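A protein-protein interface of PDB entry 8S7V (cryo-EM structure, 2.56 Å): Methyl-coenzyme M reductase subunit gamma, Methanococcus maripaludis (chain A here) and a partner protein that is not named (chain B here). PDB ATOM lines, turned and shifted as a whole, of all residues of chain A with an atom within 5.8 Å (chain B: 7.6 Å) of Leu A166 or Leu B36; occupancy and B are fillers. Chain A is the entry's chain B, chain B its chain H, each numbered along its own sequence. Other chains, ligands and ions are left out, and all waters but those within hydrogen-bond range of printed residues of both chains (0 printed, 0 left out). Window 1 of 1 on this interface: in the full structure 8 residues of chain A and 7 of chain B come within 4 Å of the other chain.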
ATOM      1  N   SER A  93       6.702   8.292  -9.672  1.00  0.00           N
ATOM      2  CA  SER A  93       6.834   7.942 -11.076  1.00  0.00           C
ATOM      3  C   SER A  93       6.274   9.046 -11.963  1.00  0.00           C
ATOM      4  O   SER A  93       5.302   9.720 -11.617  1.00  0.00           O
ATOM      5  CB  SER A  93       6.116   6.628 -11.373  1.00  0.00           C
ATOM      6  OG  SER A  93       6.131   6.345 -12.758  1.00  0.00           O
ATOM      7  N   TYR A  95       4.743   8.469 -14.583  1.00  0.00           N
ATOM      8  CA  TYR A  95       3.542   7.915 -15.207  1.00  0.00           C
ATOM      9  C   TYR A  95       2.363   7.991 -14.235  1.00  0.00           C
ATOM     10  O   TYR A  95       1.948   7.008 -13.618  1.00  0.00           O
ATOM     11  CB  TYR A  95       3.799   6.489 -15.673  1.00  0.00           C
ATOM     12  CG  TYR A  95       4.829   6.398 -16.772  1.00  0.00           C
ATOM     13  CD1 TYR A  95       4.459   6.501 -18.104  1.00  0.00           C
ATOM     14  CD2 TYR A  95       6.172   6.214 -16.478  1.00  0.00           C
ATOM     15  CE1 TYR A  95       5.395   6.421 -19.112  1.00  0.00           C
ATOM     16  CE2 TYR A  95       7.115   6.136 -17.480  1.00  0.00           C
ATOM     17  CZ  TYR A  95       6.721   6.240 -18.795  1.00  0.00           C
ATOM     18  OH  TYR A  95       7.657   6.161 -19.797  1.00  0.00           O
ATOM     19  N   ALA A 150       2.062   1.533  -5.893  1.00  0.00           N
ATOM     20  CA  ALA A 150       2.667   1.090  -7.145  1.00  0.00           C
ATOM     21  C   ALA A 150       3.527   2.181  -7.779  1.00  0.00           C
ATOM     22  O   ALA A 150       4.719   1.975  -8.023  1.00  0.00           O
ATOM     23  CB  ALA A 150       1.578   0.634  -8.120  1.00  0.00           C
ATOM     24  N   THR A 151       2.935   3.344  -8.052  1.00  0.00           N
ATOM     25  CA  THR A 151       3.637   4.407  -8.758  1.00  0.00           C
ATOM     26  C   THR A 151       4.486   5.282  -7.846  1.00  0.00           C
ATOM     27  O   THR A 151       5.288   6.073  -8.351  1.00  0.00           O
ATOM     28  CB  THR A 151       2.640   5.288  -9.511  1.00  0.00           C
ATOM     29  OG1 THR A 151       1.592   5.692  -8.624  1.00  0.00           O
ATOM     30  CG2 THR A 151       2.039   4.528 -10.678  1.00  0.00           C
ATOM     31  N   LEU A 164      11.692   5.919 -15.622  1.00  0.00           N
ATOM     32  CA  LEU A 164      11.613   4.642 -16.308  1.00  0.00           C
ATOM     33  C   LEU A 164      10.163   4.186 -16.422  1.00  0.00           C
ATOM     34  O   LEU A 164       9.267   4.697 -15.746  1.00  0.00           O
ATOM     35  CB  LEU A 164      12.435   3.583 -15.577  1.00  0.00           C
ATOM     36  CG  LEU A 164      13.885   3.938 -15.258  1.00  0.00           C
ATOM     37  CD1 LEU A 164      14.588   2.758 -14.619  1.00  0.00           C
ATOM     38  CD2 LEU A 164      14.614   4.383 -16.511  1.00  0.00           C
ATOM     39  N   ARG A 165       9.938   3.212 -17.296  1.00  0.00           N
ATOM     40  CA  ARG A 165       8.604   2.660 -17.458  1.00  0.00           C
ATOM     41  C   ARG A 165       8.269   1.722 -16.302  1.00  0.00           C
ATOM     42  O   ARG A 165       9.148   1.206 -15.608  1.00  0.00           O
ATOM     43  CB  ARG A 165       8.489   1.918 -18.788  1.00  0.00           C
ATOM     44  CG  ARG A 165       8.471   2.825 -20.003  1.00  0.00           C
ATOM     45  CD  ARG A 165       8.822   2.055 -21.259  1.00  0.00           C
ATOM     46  NE  ARG A 165      10.140   1.444 -21.166  1.00  0.00           N
ATOM     47  CZ  ARG A 165      10.648   0.617 -22.069  1.00  0.00           C
ATOM     48  NH1 ARG A 165       9.971   0.278 -23.153  1.00  0.00           N
ATOM     49  NH2 ARG A 165      11.866   0.119 -21.880  1.00  0.00           N
ATOM     50  N   LEU A 166       6.974   1.510 -16.099  1.00  0.00           N
ATOM     51  CA  LEU A 166       6.516   0.630 -15.036  1.00  0.00           C
ATOM     52  C   LEU A 166       6.767  -0.829 -15.407  1.00  0.00           C
ATOM     53  O   LEU A 166       6.936  -1.181 -16.577  1.00  0.00           O
ATOM     54  CB  LEU A 166       5.032   0.861 -14.760  1.00  0.00           C
ATOM     55  CG  LEU A 166       4.602   2.327 -14.684  1.00  0.00           C
ATOM     56  CD1 LEU A 166       3.092   2.442 -14.621  1.00  0.00           C
ATOM     57  CD2 LEU A 166       5.240   3.012 -13.492  1.00  0.00           C
ATOM     58  N   ASP A 167       6.797  -1.683 -14.388  1.00  0.00           N
ATOM     59  CA  ASP A 167       7.029  -3.107 -14.597  1.00  0.00           C
ATOM     60  C   ASP A 167       5.710  -3.797 -14.947  1.00  0.00           C
ATOM     61  O   ASP A 167       4.696  -3.151 -15.220  1.00  0.00           O
ATOM     62  CB  ASP A 167       7.752  -3.708 -13.387  1.00  0.00           C
ATOM     63  CG  ASP A 167       6.881  -3.804 -12.135  1.00  0.00           C
ATOM     64  OD1 ASP A 167       5.644  -3.942 -12.222  1.00  0.00           O
ATOM     65  OD2 ASP A 167       7.459  -3.746 -11.030  1.00  0.00           O
ATOM     66  N   GLU A 168       5.713  -5.134 -14.943  1.00  0.00           N
ATOM     67  CA  GLU A 168       4.554  -5.881 -15.419  1.00  0.00           C
ATOM     68  C   GLU A 168       3.331  -5.710 -14.528  1.00  0.00           C
ATOM     69  O   GLU A 168       2.211  -5.965 -14.985  1.00  0.00           O
ATOM     70  CB  GLU A 168       4.897  -7.366 -15.542  1.00  0.00           C
ATOM     71  CG  GLU A 168       5.088  -8.083 -14.217  1.00  0.00           C
ATOM     72  CD  GLU A 168       6.521  -8.034 -13.732  1.00  0.00           C
ATOM     73  OE1 GLU A 168       7.417  -7.743 -14.552  1.00  0.00           O
ATOM     74  OE2 GLU A 168       6.755  -8.294 -12.532  1.00  0.00           O
ATOM     75  N   GLY A 170       2.589  -2.740 -13.029  1.00  0.00           N
ATOM     76  CA  GLY A 170       2.336  -1.322 -12.899  1.00  0.00           C
ATOM     77  C   GLY A 170       3.098  -0.640 -11.790  1.00  0.00           C
ATOM     78  O   GLY A 170       2.749   0.487 -11.424  1.00  0.00           O
ATOM     79  N   MET A 171       4.123  -1.283 -11.246  1.00  0.00           N
ATOM     80  CA  MET A 171       4.897  -0.735 -10.146  1.00  0.00           C
ATOM     81  C   MET A 171       6.139  -0.020 -10.666  1.00  0.00           C
ATOM     82  O   MET A 171       6.730  -0.405 -11.676  1.00  0.00           O
ATOM     83  CB  MET A 171       5.300  -1.842  -9.173  1.00  0.00           C
ATOM     84  CG  MET A 171       4.198  -2.256  -8.215  1.00  0.00           C
ATOM     85  SD  MET A 171       4.819  -3.047  -6.720  1.00  0.00           S
ATOM     86  CE  MET A 171       6.451  -2.325  -6.603  1.00  0.00           C
ATOM     87  N   MET A 172       6.525   1.039  -9.961  1.00  0.00           N
ATOM     88  CA  MET A 172       7.734   1.766 -10.312  1.00  0.00           C
ATOM     89  C   MET A 172       8.960   0.885 -10.111  1.00  0.00           C
ATOM     90  O   MET A 172       8.993   0.017  -9.236  1.00  0.00           O
ATOM     91  CB  MET A 172       7.863   3.036  -9.472  1.00  0.00           C
ATOM     92  CG  MET A 172       8.737   4.105 -10.107  1.00  0.00           C
ATOM     93  SD  MET A 172       8.859   5.618  -9.137  1.00  0.00           S
ATOM     94  CE  MET A 172       8.457   5.011  -7.503  1.00  0.00           C
ATOM     95  N   PHE A 173       9.972   1.111 -10.942  1.00  0.00           N
ATOM     96  CA  PHE A 173      11.201   0.341 -10.841  1.00  0.00           C
ATOM     97  C   PHE A 173      11.913   0.642  -9.529  1.00  0.00           C
ATOM     98  O   PHE A 173      12.009   1.796  -9.104  1.00  0.00           O
ATOM     99  CB  PHE A 173      12.119   0.651 -12.022  1.00  0.00           C
ATOM    100  CG  PHE A 173      13.454  -0.025 -11.942  1.00  0.00           C
ATOM    101  CD1 PHE A 173      13.593  -1.353 -12.300  1.00  0.00           C
ATOM    102  CD2 PHE A 173      14.571   0.665 -11.507  1.00  0.00           C
ATOM    103  CE1 PHE A 173      14.817  -1.979 -12.224  1.00  0.00           C
ATOM    104  CE2 PHE A 173      15.797   0.042 -11.428  1.00  0.00           C
ATOM    105  CZ  PHE A 173      15.921  -1.280 -11.789  1.00  0.00           C
ATOM    106  N   GLY B   9       8.779  -4.104 -27.078  1.00  0.00           N
ATOM    107  CA  GLY B   9       8.015  -3.186 -26.258  1.00  0.00           C
ATOM    108  C   GLY B   9       8.358  -3.317 -24.792  1.00  0.00           C
ATOM    109  O   GLY B   9       9.383  -3.908 -24.444  1.00  0.00           O
ATOM    110  N   GLY B  10       7.512  -2.776 -23.922  1.00  0.00           N
ATOM    111  CA  GLY B  10       7.730  -2.846 -22.497  1.00  0.00           C
ATOM    112  C   GLY B  10       6.993  -4.005 -21.857  1.00  0.00           C
ATOM    113  O   GLY B  10       6.091  -4.596 -22.442  1.00  0.00           O
ATOM    114  N   VAL B  11       7.393  -4.325 -20.625  1.00  0.00           N
ATOM    115  CA  VAL B  11       6.751  -5.413 -19.895  1.00  0.00           C
ATOM    116  C   VAL B  11       5.415  -4.994 -19.306  1.00  0.00           C
ATOM    117  O   VAL B  11       4.597  -5.860 -18.972  1.00  0.00           O
ATOM    118  CB  VAL B  11       7.665  -5.937 -18.779  1.00  0.00           C
ATOM    119  CG1 VAL B  11       8.886  -6.594 -19.377  1.00  0.00           C
ATOM    120  CG2 VAL B  11       8.066  -4.809 -17.850  1.00  0.00           C
ATOM    121  N   TYR B  12       5.168  -3.695 -19.168  1.00  0.00           N
ATOM    122  CA  TYR B  12       3.901  -3.227 -18.629  1.00  0.00           C
ATOM    123  C   TYR B  12       2.777  -3.517 -19.614  1.00  0.00           C
ATOM    124  O   TYR B  12       2.864  -3.163 -20.793  1.00  0.00           O
ATOM    125  CB  TYR B  12       3.977  -1.732 -18.330  1.00  0.00           C
ATOM    126  CG  TYR B  12       2.731  -1.162 -17.699  1.00  0.00           C
ATOM    127  CD1 TYR B  12       2.072  -1.840 -16.685  1.00  0.00           C
ATOM    128  CD2 TYR B  12       2.219   0.058 -18.111  1.00  0.00           C
ATOM    129  CE1 TYR B  12       0.933  -1.322 -16.106  1.00  0.00           C
ATOM    130  CE2 TYR B  12       1.083   0.584 -17.537  1.00  0.00           C
ATOM    131  CZ  TYR B  12       0.444  -0.110 -16.535  1.00  0.00           C
ATOM    132  OH  TYR B  12      -0.688   0.411 -15.958  1.00  0.00           O
ATOM    133  N   LYS B  13       1.722  -4.172 -19.124  1.00  0.00           N
ATOM    134  CA  LYS B  13       0.564  -4.554 -19.935  1.00  0.00           C
ATOM    135  C   LYS B  13       0.953  -5.468 -21.094  1.00  0.00           C
ATOM    136  O   LYS B  13       0.242  -5.550 -22.098  1.00  0.00           O
ATOM    137  CB  LYS B  13      -0.186  -3.325 -20.455  1.00  0.00           C
ATOM    138  CG  LYS B  13      -0.592  -2.343 -19.375  1.00  0.00           C
ATOM    139  CD  LYS B  13      -1.937  -1.717 -19.683  1.00  0.00           C
ATOM    140  CE  LYS B  13      -1.777  -0.291 -20.179  1.00  0.00           C
ATOM    141  NZ  LYS B  13      -2.120   0.704 -19.128  1.00  0.00           N
ATOM    142  N   HIS B  32      11.855 -12.681 -24.113  1.00  0.00           N
ATOM    143  CA  HIS B  32      12.980 -12.315 -23.264  1.00  0.00           C
ATOM    144  C   HIS B  32      12.729 -10.935 -22.678  1.00  0.00           C
ATOM    145  O   HIS B  32      12.414  -9.996 -23.413  1.00  0.00           O
ATOM    146  CB  HIS B  32      14.298 -12.334 -24.044  1.00  0.00           C
ATOM    147  CG  HIS B  32      15.510 -12.432 -23.171  1.00  0.00           C
ATOM    148  ND1 HIS B  32      16.427 -11.410 -23.053  1.00  0.00           N
ATOM    149  CD2 HIS B  32      15.953 -13.430 -22.371  1.00  0.00           C
ATOM    150  CE1 HIS B  32      17.383 -11.775 -22.217  1.00  0.00           C
ATOM    151  NE2 HIS B  32      17.118 -12.996 -21.790  1.00  0.00           N
ATOM    152  N   VAL B  33      12.871 -10.823 -21.363  1.00  0.00           N
ATOM    153  CA  VAL B  33      12.688  -9.571 -20.638  1.00  0.00           C
ATOM    154  C   VAL B  33      14.047  -9.141 -20.111  1.00  0.00           C
ATOM    155  O   VAL B  33      14.662  -9.861 -19.315  1.00  0.00           O
ATOM    156  CB  VAL B  33      11.680  -9.730 -19.489  1.00  0.00           C
ATOM    157  CG1 VAL B  33      11.746  -8.535 -18.559  1.00  0.00           C
ATOM    158  CG2 VAL B  33      10.277  -9.925 -20.034  1.00  0.00           C
ATOM    159  N   MET B  34      14.527  -7.977 -20.550  1.00  0.00           N
ATOM    160  CA  MET B  34      15.869  -7.567 -20.139  1.00  0.00           C
ATOM    161  C   MET B  34      15.842  -6.910 -18.761  1.00  0.00           C
ATOM    162  O   MET B  34      16.299  -7.494 -17.773  1.00  0.00           O
ATOM    163  CB  MET B  34      16.466  -6.611 -21.177  1.00  0.00           C
ATOM    164  CG  MET B  34      16.803  -7.245 -22.515  1.00  0.00           C
ATOM    165  SD  MET B  34      15.390  -7.237 -23.634  1.00  0.00           S
ATOM    166  CE  MET B  34      15.686  -8.719 -24.586  1.00  0.00           C
ATOM    167  N   GLN B  35      15.297  -5.696 -18.675  1.00  0.00           N
ATOM    168  CA  GLN B  35      15.006  -5.081 -17.386  1.00  0.00           C
ATOM    169  C   GLN B  35      13.544  -4.665 -17.313  1.00  0.00           C
ATOM    170  O   GLN B  35      12.811  -5.071 -16.407  1.00  0.00           O
ATOM    171  CB  GLN B  35      15.922  -3.880 -17.147  1.00  0.00           C
ATOM    172  CG  GLN B  35      15.391  -2.882 -16.136  1.00  0.00           C
ATOM    173  CD  GLN B  35      16.304  -1.689 -15.967  1.00  0.00           C
ATOM    174  OE1 GLN B  35      17.380  -1.631 -16.557  1.00  0.00           O
ATOM    175  NE2 GLN B  35      15.878  -0.725 -15.163  1.00  0.00           N
ATOM    176  N   LEU B  36      13.118  -3.860 -18.288  1.00  0.00           N
ATOM    177  CA  LEU B  36      11.746  -3.391 -18.391  1.00  0.00           C
ATOM    178  C   LEU B  36      11.183  -3.508 -19.794  1.00  0.00           C
ATOM    179  O   LEU B  36      10.009  -3.179 -19.996  1.00  0.00           O
ATOM    180  CB  LEU B  36      11.634  -1.925 -17.940  1.00  0.00           C
ATOM    181  CG  LEU B  36      11.835  -1.615 -16.459  1.00  0.00           C
ATOM    182  CD1 LEU B  36      12.305  -0.184 -16.282  1.00  0.00           C
ATOM    183  CD2 LEU B  36      10.555  -1.857 -15.683  1.00  0.00           C
ATOM    184  N   ASP B  37      11.974  -3.948 -20.764  1.00  0.00           N
ATOM    185  CA  ASP B  37      11.520  -4.148 -22.128  1.00  0.00           C
ATOM    186  C   ASP B  37      11.553  -5.631 -22.465  1.00  0.00           C
ATOM    187  O   ASP B  37      12.423  -6.372 -22.001  1.00  0.00           O
ATOM    188  CB  ASP B  37      12.378  -3.357 -23.119  1.00  0.00           C
ATOM    189  CG  ASP B  37      13.844  -3.342 -22.742  1.00  0.00           C
ATOM    190  OD1 ASP B  37      14.315  -4.318 -22.124  1.00  0.00           O
ATOM    191  OD2 ASP B  37      14.530  -2.349 -23.063  1.00  0.00           O
ATOM    192  N   VAL B  38      10.589  -6.060 -23.272  1.00  0.00           N
ATOM    193  CA  VAL B  38      10.420  -7.463 -23.625  1.00  0.00           C
ATOM    194  C   VAL B  38      10.473  -7.585 -25.141  1.00  0.00           C
ATOM    195  O   VAL B  38       9.850  -6.793 -25.856  1.00  0.00           O
ATOM    196  CB  VAL B  38       9.103  -8.033 -23.065  1.00  0.00           C
ATOM    197  CG1 VAL B  38       7.936  -7.126 -23.407  1.00  0.00           C
ATOM    198  CG2 VAL B  38       8.863  -9.439 -23.583  1.00  0.00           C
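The guanidinium group of Arg A165 lies within salt-bridge range of the side-chain carboxylate of Asp B37.
The side-chain carboxylate of Asp A167 is in hydrogen-bond range of the backbone NH of Gly A170 (3.4 Å).
N of Met A171 is in hydrogen-bond range of OD1 of Asp A167 (3.2 Å).
The backbone NH (N) of Val B11 lies within hydrogen-bond range of the backbone carbonyl oxygen (O) of Leu B36.
The side-chain hydroxyl (OH) of Tyr B12 lies within hydrogen-bond range of the side-chain amino group (NZ) of Lys B13 (3.5 Å).
Leu A164 touches Gln B35.
Leu A164 touches Leu B36 (CB to CD1, 3.8 Å).
CA of Gly B10 touches NH1 of Arg A165 (3.9 Å).
Leu B36 touches Arg A165.
Leu A166 touches Tyr B12.
CD2 of Leu B36 touches O of Leu A166, 3.8 Å away.
CD1 of Tyr B12 touches O of Asp A167 (3.3 Å).
Leu B36 touches Asp A167 (CD2 to CA, 3.9 Å).
Val B11 touches Glu A168 (O to CA, 3.6 Å).
Phe A173 touches Gln B35.
Thr A151 touches none of the printed residues of chain B.
Printed residues of chain B within 4 Å of Glu A168: Val B11 (3.6 Å).
Printed residues of chain B within 4 Å of Phe A173: Gln B35.
Of the printed residues of chain A, Gly B10 touches Arg A165 (3.9 Å).
Of the printed residues of chain A, Gln B35 touches Leu A164 (3.8 Å) and Phe A173 (3.4 Å).
Leu B36 touches four residues of chain A.
Val B38 touches none of the printed residues of chain A.
Of the 12 printed residues of chain B, 6 touch a printed residue of chain A.
Hydrophobic or aromatic side chains of chain B within 4 Å of the printed part of chain A: Val B11, Tyr B12 and Leu B36.
Of the 13 printed residues of chain A, 7 touch a printed residue of chain B.
Printed residues of chain A that touch a printed residue of chain B: Leu A164, Arg A165, Leu A166, Asp A167, Glu A168, Gly A170 and Phe A173.
Hydrophobic or aromatic side chains of chain A within 4 Å of the printed part of chain B: Leu A164, Leu A166 and Phe A173.
Among the printed residues, 13 pairs touch across the chains.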
